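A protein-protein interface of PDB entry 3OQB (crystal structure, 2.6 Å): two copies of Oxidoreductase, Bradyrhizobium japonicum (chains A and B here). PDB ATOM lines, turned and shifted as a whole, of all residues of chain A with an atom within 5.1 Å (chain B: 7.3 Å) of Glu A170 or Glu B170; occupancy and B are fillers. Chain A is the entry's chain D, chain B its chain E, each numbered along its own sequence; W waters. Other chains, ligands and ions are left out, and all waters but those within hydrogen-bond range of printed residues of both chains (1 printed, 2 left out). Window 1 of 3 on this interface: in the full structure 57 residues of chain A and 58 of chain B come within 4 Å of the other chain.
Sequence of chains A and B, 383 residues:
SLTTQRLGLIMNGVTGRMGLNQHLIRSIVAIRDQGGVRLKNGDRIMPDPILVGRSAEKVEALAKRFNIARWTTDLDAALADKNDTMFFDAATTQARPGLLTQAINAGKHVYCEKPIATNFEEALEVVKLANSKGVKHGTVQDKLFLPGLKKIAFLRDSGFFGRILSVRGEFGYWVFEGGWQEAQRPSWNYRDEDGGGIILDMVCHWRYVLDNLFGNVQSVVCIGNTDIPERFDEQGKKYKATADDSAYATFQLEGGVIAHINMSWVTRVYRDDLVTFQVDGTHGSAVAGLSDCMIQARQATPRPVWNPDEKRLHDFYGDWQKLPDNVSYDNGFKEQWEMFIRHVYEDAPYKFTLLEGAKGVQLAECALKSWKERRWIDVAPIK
Of the 20 printed residues of chain B, 5 touch a printed residue of chain A. Hydrophobic or aromatic side chains of chain B that line the printed part of chain A: His B260. Along chain B the printed residues that touch a printed residue of chain A span positions 168 to 267. Printed residues of chain A that touch a printed residue of chain B: Arg A168, Glu A170 and Asn A262. Along chain A the printed residues that touch a printed residue of chain B span positions 168 to 262. Among the printed residues, no Asp or Glu carboxylate lies within 4 Å of a Lys or Arg side-chain nitrogen of the other chain.
Arg A168 touches Glu B170 (CD to OE1, 3.8 Å). ND2 of Asn B262 touches CG of Arg A168, at 3.5 Å. Thr B267 touches Arg A168. Glu A170 touches Arg B168 (OE1 to CD, 3.7 Å). ND2 of Asn A262 touches CG of Arg B168, at 3.4 Å. Asn A262 touches His B260.
Water W1 lies within hydrogen-bond range of the backbone carbonyl oxygen of Phe A171 (2.6 Å), the guanidinium group of Arg B168 (2.7 Å) and the backbone carbonyl oxygen of Asn A262 (3.0 Å).
Arg A168 touches Glu B170, and with the chains exchanged Glu A170 touches Arg B168. Arg A168 touches Asn B262, and with the chains exchanged Asn A262 touches Arg B168. Glu A170 touches its own counterpart, Glu B170. Positions printed for both chains: 168, 169, 170, 171, 172, 261, 262, 271, 274, 275 and 276. Of the 7 pairs that touch across the chains among the printed residues, 5 have their exchanged pair printed and touching as well.
OE2 of Glu A170 sits close to OE2 of Glu B170 (3.3 Å).
N of Asn A262 sits at hydrogen-bond distance from O of Gly A169 (3.0 Å). The side-chain carboxylate (OE2) of Glu B170 is in hydrogen-bond range of the side-chain amide nitrogen (ND2) of Asn B262 (2.9 Å). OE2 of Glu A170 lies within hydrogen-bond range of ND2 of Asn A262 (3.1 Å). N of Gly B169 is in hydrogen-bond range of O of His B260 (2.7 Å). The backbone NH of Phe A171 is in hydrogen-bond range of the backbone carbonyl oxygen of Asn A262 (2.8 Å). The backbone carbonyl oxygen of Thr B276 lies within hydrogen-bond range of the backbone NH of Glu B170.
Glu A170 touches two residues of chain B. Printed residues of chain B within 4 Å of Asn A262: Arg B168 and His B260. Of chain A, only Arg A168 and Glu A170 come within 4 Å of Glu B170. Printed residues of chain A within 4 Å of His B260: Asn A262 (3.8 Å). Printed residues of chain A within 4 Å of Asn B262: Arg A168. Printed residues of chain A within 4 Å of Thr B267: Arg A168. The nearest residue of chain A that does not touch Glu B170 is Asn A262 (4.8 Å). The nearest printed residue of chain B that does not touch Arg A168 is Ser B264 (4.1 Å).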
ATOM      1  N   ARG A 168      -7.513  10.494  14.990  1.00  0.00           N
ATOM      2  CA  ARG A 168      -7.048  11.840  15.305  1.00  0.00           C
ATOM      3  C   ARG A 168      -5.555  11.832  15.447  1.00  0.00           C
ATOM      4  O   ARG A 168      -5.011  11.088  16.254  1.00  0.00           O
ATOM      5  CB  ARG A 168      -7.674  12.330  16.604  1.00  0.00           C
ATOM      6  CG  ARG A 168      -8.964  13.103  16.406  1.00  0.00           C
ATOM      7  CD  ARG A 168      -9.899  12.938  17.586  1.00  0.00           C
ATOM      8  NE  ARG A 168     -11.004  12.075  17.210  1.00  0.00           N
ATOM      9  CZ  ARG A 168     -12.279  12.419  17.287  1.00  0.00           C
ATOM     10  NH1 ARG A 168     -13.195  11.559  16.901  1.00  0.00           N
ATOM     11  NH2 ARG A 168     -12.638  13.604  17.762  1.00  0.00           N
ATOM     12  N   GLY A 169      -4.883  12.639  14.640  1.00  0.00           N
ATOM     13  CA  GLY A 169      -3.443  12.731  14.679  1.00  0.00           C
ATOM     14  C   GLY A 169      -3.048  14.125  15.104  1.00  0.00           C
ATOM     15  O   GLY A 169      -3.630  15.116  14.664  1.00  0.00           O
ATOM     16  N   GLU A 170      -2.048  14.205  15.967  1.00  0.00           N
ATOM     17  CA  GLU A 170      -1.571  15.478  16.438  1.00  0.00           C
ATOM     18  C   GLU A 170      -0.086  15.403  16.267  1.00  0.00           C
ATOM     19  O   GLU A 170       0.569  14.658  16.992  1.00  0.00           O
ATOM     20  CB  GLU A 170      -1.943  15.673  17.907  1.00  0.00           C
ATOM     21  CG  GLU A 170      -3.435  15.917  18.155  1.00  0.00           C
ATOM     22  CD  GLU A 170      -3.944  17.269  17.616  1.00  0.00           C
ATOM     23  OE1 GLU A 170      -3.113  18.186  17.317  1.00  0.00           O
ATOM     24  OE2 GLU A 170      -5.197  17.401  17.515  1.00  0.00           O
ATOM     25  N   PHE A 171       0.449  16.138  15.288  1.00  0.00           N
ATOM     26  CA  PHE A 171       1.863  16.017  14.960  1.00  0.00           C
ATOM     27  C   PHE A 171       2.646  17.299  15.062  1.00  0.00           C
ATOM     28  O   PHE A 171       2.226  18.350  14.537  1.00  0.00           O
ATOM     29  CB  PHE A 171       2.117  15.423  13.562  1.00  0.00           C
ATOM     30  CG  PHE A 171       3.562  15.535  13.145  1.00  0.00           C
ATOM     31  CD1 PHE A 171       4.478  14.570  13.526  1.00  0.00           C
ATOM     32  CD2 PHE A 171       4.013  16.648  12.447  1.00  0.00           C
ATOM     33  CE1 PHE A 171       5.800  14.671  13.189  1.00  0.00           C
ATOM     34  CE2 PHE A 171       5.348  16.786  12.110  1.00  0.00           C
ATOM     35  CZ  PHE A 171       6.255  15.795  12.480  1.00  0.00           C
ATOM     36  N   GLY A 172       3.823  17.184  15.676  1.00  0.00           N
ATOM     37  CA  GLY A 172       4.770  18.282  15.693  1.00  0.00           C
ATOM     38  C   GLY A 172       5.175  18.815  17.055  1.00  0.00           C
ATOM     39  O   GLY A 172       4.918  18.202  18.097  1.00  0.00           O
ATOM     40  N   ILE A 261      -5.590  15.083  10.769  1.00  0.00           N
ATOM     41  CA  ILE A 261      -4.269  15.287  11.331  1.00  0.00           C
ATOM     42  C   ILE A 261      -3.914  16.758  11.337  1.00  0.00           C
ATOM     43  O   ILE A 261      -3.874  17.399  10.283  1.00  0.00           O
ATOM     44  CB  ILE A 261      -3.170  14.532  10.567  1.00  0.00           C
ATOM     45  CG1 ILE A 261      -3.554  13.068  10.396  1.00  0.00           C
ATOM     46  CG2 ILE A 261      -1.870  14.658  11.316  1.00  0.00           C
ATOM     47  CD1 ILE A 261      -2.515  12.225   9.726  1.00  0.00           C
ATOM     48  N   ASN A 262      -3.678  17.287  12.535  1.00  0.00           N
ATOM     49  CA  ASN A 262      -3.001  18.557  12.682  1.00  0.00           C
ATOM     50  C   ASN A 262      -1.488  18.318  12.647  1.00  0.00           C
ATOM     51  O   ASN A 262      -0.983  17.376  13.253  1.00  0.00           O
ATOM     52  CB  ASN A 262      -3.423  19.232  13.975  1.00  0.00           C
ATOM     53  CG  ASN A 262      -4.913  19.568  14.012  1.00  0.00           C
ATOM     54  OD1 ASN A 262      -5.501  20.045  13.018  1.00  0.00           O
ATOM     55  ND2 ASN A 262      -5.531  19.347  15.184  1.00  0.00           N
ATOM     56  N   ARG A 271       0.888  16.604  25.235  1.00  0.00           N
ATOM     57  CA  ARG A 271       0.435  15.271  24.862  1.00  0.00           C
ATOM     58  C   ARG A 271       1.551  14.280  25.163  1.00  0.00           C
ATOM     59  O   ARG A 271       2.665  14.685  25.446  1.00  0.00           O
ATOM     60  CB  ARG A 271       0.027  15.218  23.387  1.00  0.00           C
ATOM     61  CG  ARG A 271       0.943  15.925  22.418  1.00  0.00           C
ATOM     62  CD  ARG A 271       0.433  15.728  20.954  1.00  0.00           C
ATOM     63  NE  ARG A 271       0.727  16.913  20.143  1.00  0.00           N
ATOM     64  CZ  ARG A 271       1.899  17.180  19.573  1.00  0.00           C
ATOM     65  NH1 ARG A 271       2.044  18.314  18.905  1.00  0.00           N
ATOM     66  NH2 ARG A 271       2.922  16.327  19.658  1.00  0.00           N
ATOM     67  N   LEU A 274       5.831  13.361  20.676  1.00  0.00           N
ATOM     68  CA  LEU A 274       6.031  14.275  19.545  1.00  0.00           C
ATOM     69  C   LEU A 274       5.014  14.044  18.429  1.00  0.00           C
ATOM     70  O   LEU A 274       4.725  14.973  17.673  1.00  0.00           O
ATOM     71  CB  LEU A 274       7.473  14.253  19.025  1.00  0.00           C
ATOM     72  CG  LEU A 274       8.578  14.624  20.018  1.00  0.00           C
ATOM     73  CD1 LEU A 274       9.956  14.675  19.338  1.00  0.00           C
ATOM     74  CD2 LEU A 274       8.273  15.941  20.704  1.00  0.00           C
ATOM     75  N   VAL A 275       4.451  12.824  18.368  1.00  0.00           N
ATOM     76  CA  VAL A 275       3.217  12.560  17.601  1.00  0.00           C
ATOM     77  C   VAL A 275       2.241  11.685  18.412  1.00  0.00           C
ATOM     78  O   VAL A 275       2.639  10.953  19.310  1.00  0.00           O
ATOM     79  CB  VAL A 275       3.499  11.965  16.177  1.00  0.00           C
ATOM     80  CG1 VAL A 275       3.931  10.517  16.243  1.00  0.00           C
ATOM     81  CG2 VAL A 275       2.270  12.082  15.292  1.00  0.00           C
ATOM     82  N   THR A 276       0.965  11.754  18.068  1.00  0.00           N
ATOM     83  CA  THR A 276      -0.078  11.094  18.827  1.00  0.00           C
ATOM     84  C   THR A 276      -1.160  10.680  17.854  1.00  0.00           C
ATOM     85  O   THR A 276      -1.613  11.488  17.049  1.00  0.00           O
ATOM     86  CB  THR A 276      -0.618  12.081  19.914  1.00  0.00           C
ATOM     87  OG1 THR A 276      -0.123  11.687  21.207  1.00  0.00           O
ATOM     88  CG2 THR A 276      -2.154  12.193  19.937  1.00  0.00           C
ATOM     89  N   ARG B 168      -6.573  24.746  18.264  1.00  0.00           N
ATOM     90  CA  ARG B 168      -6.955  23.338  18.137  1.00  0.00           C
ATOM     91  C   ARG B 168      -8.001  23.067  19.165  1.00  0.00           C
ATOM     92  O   ARG B 168      -7.725  23.202  20.363  1.00  0.00           O
ATOM     93  CB  ARG B 168      -5.776  22.423  18.443  1.00  0.00           C
ATOM     94  CG  ARG B 168      -5.011  21.946  17.265  1.00  0.00           C
ATOM     95  CD  ARG B 168      -3.527  21.870  17.579  1.00  0.00           C
ATOM     96  NE  ARG B 168      -2.848  22.964  16.900  1.00  0.00           N
ATOM     97  CZ  ARG B 168      -1.900  22.810  15.988  1.00  0.00           C
ATOM     98  NH1 ARG B 168      -1.355  23.879  15.415  1.00  0.00           N
ATOM     99  NH2 ARG B 168      -1.486  21.599  15.643  1.00  0.00           N
ATOM    100  N   GLY B 169      -9.189  22.692  18.723  1.00  0.00           N
ATOM    101  CA  GLY B 169     -10.286  22.375  19.643  1.00  0.00           C
ATOM    102  C   GLY B 169     -10.635  20.897  19.611  1.00  0.00           C
ATOM    103  O   GLY B 169     -10.721  20.296  18.524  1.00  0.00           O
ATOM    104  N   GLU B 170     -10.807  20.310  20.799  1.00  0.00           N
ATOM    105  CA  GLU B 170     -11.213  18.910  20.961  1.00  0.00           C
ATOM    106  C   GLU B 170     -12.441  18.847  21.835  1.00  0.00           C
ATOM    107  O   GLU B 170     -12.387  19.183  23.011  1.00  0.00           O
ATOM    108  CB  GLU B 170     -10.107  18.086  21.632  1.00  0.00           C
ATOM    109  CG  GLU B 170      -8.830  17.963  20.840  1.00  0.00           C
ATOM    110  CD  GLU B 170      -9.001  17.110  19.593  1.00  0.00           C
ATOM    111  OE1 GLU B 170      -9.783  16.101  19.639  1.00  0.00           O
ATOM    112  OE2 GLU B 170      -8.323  17.449  18.579  1.00  0.00           O
ATOM    113  N   PHE B 171     -13.556  18.429  21.266  1.00  0.00           N
ATOM    114  CA  PHE B 171     -14.795  18.373  22.030  1.00  0.00           C
ATOM    115  C   PHE B 171     -15.434  17.006  21.951  1.00  0.00           C
ATOM    116  O   PHE B 171     -15.398  16.342  20.901  1.00  0.00           O
ATOM    117  CB  PHE B 171     -15.811  19.424  21.561  1.00  0.00           C
ATOM    118  CG  PHE B 171     -17.162  19.230  22.156  1.00  0.00           C
ATOM    119  CD1 PHE B 171     -17.474  19.774  23.406  1.00  0.00           C
ATOM    120  CD2 PHE B 171     -18.108  18.460  21.515  1.00  0.00           C
ATOM    121  CE1 PHE B 171     -18.753  19.573  23.999  1.00  0.00           C
ATOM    122  CE2 PHE B 171     -19.360  18.250  22.080  1.00  0.00           C
ATOM    123  CZ  PHE B 171     -19.684  18.801  23.321  1.00  0.00           C
ATOM    124  N   GLY B 172     -16.035  16.599  23.062  1.00  0.00           N
ATOM    125  CA  GLY B 172     -16.868  15.401  23.060  1.00  0.00           C
ATOM    126  C   GLY B 172     -16.424  14.316  24.008  1.00  0.00           C
ATOM    127  O   GLY B 172     -15.353  14.406  24.614  1.00  0.00           O
ATOM    128  N   TRP B 206     -19.371  27.231  18.505  1.00  0.00           N
ATOM    129  CA  TRP B 206     -18.083  27.581  17.890  1.00  0.00           C
ATOM    130  C   TRP B 206     -18.031  28.945  17.188  1.00  0.00           C
ATOM    131  O   TRP B 206     -16.967  29.590  17.123  1.00  0.00           O
ATOM    132  CB  TRP B 206     -17.594  26.484  16.936  1.00  0.00           C
ATOM    133  CG  TRP B 206     -17.607  25.070  17.514  1.00  0.00           C
ATOM    134  CD1 TRP B 206     -17.848  23.924  16.824  1.00  0.00           C
ATOM    135  CD2 TRP B 206     -17.387  24.672  18.881  1.00  0.00           C
ATOM    136  NE1 TRP B 206     -17.788  22.843  17.656  1.00  0.00           N
ATOM    137  CE2 TRP B 206     -17.498  23.267  18.925  1.00  0.00           C
ATOM    138  CE3 TRP B 206     -17.097  25.358  20.063  1.00  0.00           C
ATOM    139  CZ2 TRP B 206     -17.333  22.528  20.120  1.00  0.00           C
ATOM    140  CZ3 TRP B 206     -16.936  24.628  21.246  1.00  0.00           C
ATOM    141  CH2 TRP B 206     -17.055  23.230  21.262  1.00  0.00           C
ATOM    142  N   HIS B 260      -8.961  24.620  14.119  1.00  0.00           N
ATOM    143  CA  HIS B 260      -9.552  23.330  13.826  1.00  0.00           C
ATOM    144  C   HIS B 260     -10.223  22.716  15.024  1.00  0.00           C
ATOM    145  O   HIS B 260      -9.650  22.703  16.104  1.00  0.00           O
ATOM    146  CB  HIS B 260      -8.568  22.307  13.261  1.00  0.00           C
ATOM    147  CG  HIS B 260      -9.253  21.033  12.920  1.00  0.00           C
ATOM    148  ND1 HIS B 260      -9.949  20.870  11.743  1.00  0.00           N
ATOM    149  CD2 HIS B 260      -9.490  19.926  13.656  1.00  0.00           C
ATOM    150  CE1 HIS B 260     -10.531  19.687  11.746  1.00  0.00           C
ATOM    151  NE2 HIS B 260     -10.273  19.096  12.897  1.00  0.00           N
ATOM    152  N   ILE B 261     -11.411  22.161  14.814  1.00  0.00           N
ATOM    153  CA  ILE B 261     -12.183  21.612  15.903  1.00  0.00           C
ATOM    154  C   ILE B 261     -12.689  20.240  15.537  1.00  0.00           C
ATOM    155  O   ILE B 261     -13.414  20.089  14.563  1.00  0.00           O
ATOM    156  CB  ILE B 261     -13.389  22.526  16.290  1.00  0.00           C
ATOM    157  CG1 ILE B 261     -12.905  23.936  16.674  1.00  0.00           C
ATOM    158  CG2 ILE B 261     -14.177  21.883  17.436  1.00  0.00           C
ATOM    159  CD1 ILE B 261     -14.015  24.924  16.986  1.00  0.00           C
ATOM    160  N   ASN B 262     -12.294  19.241  16.318  1.00  0.00           N
ATOM    161  CA  ASN B 262     -12.892  17.920  16.240  1.00  0.00           C
ATOM    162  C   ASN B 262     -14.027  17.906  17.217  1.00  0.00           C
ATOM    163  O   ASN B 262     -13.918  18.502  18.283  1.00  0.00           O
ATOM    164  CB  ASN B 262     -11.880  16.844  16.585  1.00  0.00           C
ATOM    165  CG  ASN B 262     -10.732  16.794  15.597  1.00  0.00           C
ATOM    166  OD1 ASN B 262     -10.938  16.962  14.406  1.00  0.00           O
ATOM    167  ND2 ASN B 262      -9.518  16.565  16.087  1.00  0.00           N
ATOM    168  N   MET B 263     -15.129  17.263  16.859  1.00  0.00           N
ATOM    169  CA  MET B 263     -16.254  17.205  17.759  1.00  0.00           C
ATOM    170  C   MET B 263     -16.961  15.875  17.609  1.00  0.00           C
ATOM    171  O   MET B 263     -17.227  15.441  16.505  1.00  0.00           O
ATOM    172  CB  MET B 263     -17.192  18.379  17.500  1.00  0.00           C
ATOM    173  CG  MET B 263     -17.770  18.380  16.093  1.00  0.00           C
ATOM    174  SD  MET B 263     -18.683  20.033  15.645  1.00  0.00           S
ATOM    175  CE  MET B 263     -17.264  20.849  14.583  1.00  0.00           C
ATOM    176  N   SER B 264     -17.272  15.222  18.718  1.00  0.00           N
ATOM    177  CA  SER B 264     -17.866  13.904  18.627  1.00  0.00           C
ATOM    178  C   SER B 264     -18.531  13.391  19.880  1.00  0.00           C
ATOM    179  O   SER B 264     -18.001  13.528  20.982  1.00  0.00           O
ATOM    180  CB  SER B 264     -16.836  12.871  18.190  1.00  0.00           C
ATOM    181  OG  SER B 264     -17.476  11.620  18.058  1.00  0.00           O
ATOM    182  N   THR B 267     -16.317   9.632  20.710  1.00  0.00           N
ATOM    183  CA  THR B 267     -14.886   9.597  20.937  1.00  0.00           C
ATOM    184  C   THR B 267     -14.632   9.333  22.423  1.00  0.00           C
ATOM    185  O   THR B 267     -15.488   9.635  23.258  1.00  0.00           O
ATOM    186  CB  THR B 267     -14.233  10.910  20.467  1.00  0.00           C
ATOM    187  OG1 THR B 267     -12.814  10.737  20.368  1.00  0.00           O
ATOM    188  CG2 THR B 267     -14.574  12.068  21.397  1.00  0.00           C
ATOM    189  N   ARG B 271      -7.528  13.499  27.541  1.00  0.00           N
ATOM    190  CA  ARG B 271      -7.194  14.909  27.585  1.00  0.00           C
ATOM    191  C   ARG B 271      -7.641  15.450  28.939  1.00  0.00           C
ATOM    192  O   ARG B 271      -8.143  14.700  29.775  1.00  0.00           O
ATOM    193  CB  ARG B 271      -7.855  15.677  26.432  1.00  0.00           C
ATOM    194  CG  ARG B 271      -9.345  15.370  26.234  1.00  0.00           C
ATOM    195  CD  ARG B 271      -9.956  16.174  25.093  1.00  0.00           C
ATOM    196  NE  ARG B 271     -10.728  15.300  24.222  1.00  0.00           N
ATOM    197  CZ  ARG B 271     -12.036  15.089  24.331  1.00  0.00           C
ATOM    198  NH1 ARG B 271     -12.649  14.273  23.483  1.00  0.00           N
ATOM    199  NH2 ARG B 271     -12.737  15.707  25.276  1.00  0.00           N
ATOM    200  N   ASP B 273     -10.121  17.636  29.773  1.00  0.00           N
ATOM    201  CA  ASP B 273     -11.551  17.892  30.027  1.00  0.00           C
ATOM    202  C   ASP B 273     -12.478  17.477  28.878  1.00  0.00           C
ATOM    203  O   ASP B 273     -12.016  17.010  27.837  1.00  0.00           O
ATOM    204  CB  ASP B 273     -11.762  19.366  30.362  1.00  0.00           C
ATOM    205  CG  ASP B 273     -12.818  19.572  31.439  1.00  0.00           C
ATOM    206  OD1 ASP B 273     -13.743  18.727  31.570  1.00  0.00           O
ATOM    207  OD2 ASP B 273     -12.724  20.591  32.154  1.00  0.00           O
ATOM    208  N   LEU B 274     -13.786  17.639  29.073  1.00  0.00           N
ATOM    209  CA  LEU B 274     -14.769  17.291  28.041  1.00  0.00           C
ATOM    210  C   LEU B 274     -14.745  18.221  26.834  1.00  0.00           C
ATOM    211  O   LEU B 274     -15.349  17.930  25.812  1.00  0.00           O
ATOM    212  CB  LEU B 274     -16.178  17.216  28.612  1.00  0.00           C
ATOM    213  CG  LEU B 274     -16.446  16.358  29.847  1.00  0.00           C
ATOM    214  CD1 LEU B 274     -17.924  16.472  30.173  1.00  0.00           C
ATOM    215  CD2 LEU B 274     -16.032  14.900  29.659  1.00  0.00           C
ATOM    216  N   VAL B 275     -14.074  19.353  26.967  1.00  0.00           N
ATOM    217  CA  VAL B 275     -13.594  20.086  25.811  1.00  0.00           C
ATOM    218  C   VAL B 275     -12.248  20.703  26.176  1.00  0.00           C
ATOM    219  O   VAL B 275     -11.963  20.973  27.341  1.00  0.00           O
ATOM    220  CB  VAL B 275     -14.566  21.168  25.319  1.00  0.00           C
ATOM    221  CG1 VAL B 275     -14.668  22.307  26.331  1.00  0.00           C
ATOM    222  CG2 VAL B 275     -14.085  21.737  24.008  1.00  0.00           C
ATOM    223  N   THR B 276     -11.436  20.944  25.155  1.00  0.00           N
ATOM    224  CA  THR B 276     -10.082  21.421  25.323  1.00  0.00           C
ATOM    225  C   THR B 276      -9.806  22.400  24.170  1.00  0.00           C
ATOM    226  O   THR B 276     -10.178  22.127  23.011  1.00  0.00           O
ATOM    227  CB  THR B 276      -9.143  20.172  25.407  1.00  0.00           C
ATOM    228  OG1 THR B 276      -8.775  19.936  26.778  1.00  0.00           O
ATOM    229  CG2 THR B 276      -7.908  20.246  24.529  1.00  0.00           C
ATOM    230  N   PHE B 277      -9.224  23.557  24.493  1.00  0.00           N
ATOM    231  CA  PHE B 277      -8.796  24.517  23.479  1.00  0.00           C
ATOM    232  C   PHE B 277      -7.315  24.830  23.639  1.00  0.00           C
ATOM    233  O   PHE B 277      -6.885  25.415  24.649  1.00  0.00           O
ATOM    234  CB  PHE B 277      -9.636  25.805  23.529  1.00  0.00           C
ATOM    235  CG  PHE B 277     -10.898  25.728  22.721  1.00  0.00           C
ATOM    236  CD1 PHE B 277     -10.862  25.864  21.339  1.00  0.00           C
ATOM    237  CD2 PHE B 277     -12.113  25.472  23.329  1.00  0.00           C
ATOM    238  CE1 PHE B 277     -12.010  25.763  20.595  1.00  0.00           C
ATOM    239  CE2 PHE B 277     -13.274  25.359  22.586  1.00  0.00           C
ATOM    240  CZ  PHE B 277     -13.232  25.498  21.229  1.00  0.00           C
ATOM    241  N   GLN B 278      -6.518  24.419  22.654  1.00  0.00           N
ATOM    242  CA  GLN B 278      -5.151  24.877  22.628  1.00  0.00           C
ATOM    243  C   GLN B 278      -5.032  26.126  21.758  1.00  0.00           C
ATOM    244  O   GLN B 278      -5.609  26.178  20.675  1.00  0.00           O
ATOM    245  CB  GLN B 278      -4.211  23.787  22.135  1.00  0.00           C
ATOM    246  CG  GLN B 278      -2.753  24.149  22.403  1.00  0.00           C
ATOM    247  CD  GLN B 278      -1.791  23.038  22.064  1.00  0.00           C
ATOM    248  OE1 GLN B 278      -2.135  21.860  22.158  1.00  0.00           O
ATOM    249  NE2 GLN B 278      -0.565  23.408  21.676  1.00  0.00           N
ATOM    250  N   ALA B 288      -6.832  25.057  27.477  1.00  0.00           N
ATOM    251  CA  ALA B 288      -7.913  25.298  28.437  1.00  0.00           C
ATOM    252  C   ALA B 288      -8.902  24.155  28.420  1.00  0.00           C
ATOM    253  O   ALA B 288      -9.106  23.523  27.395  1.00  0.00           O
ATOM    254  CB  ALA B 288      -8.620  26.617  28.148  1.00  0.00           C
HETATM  255  O   HOH W   1      -0.009  19.412  15.203  1.00  0.00           O
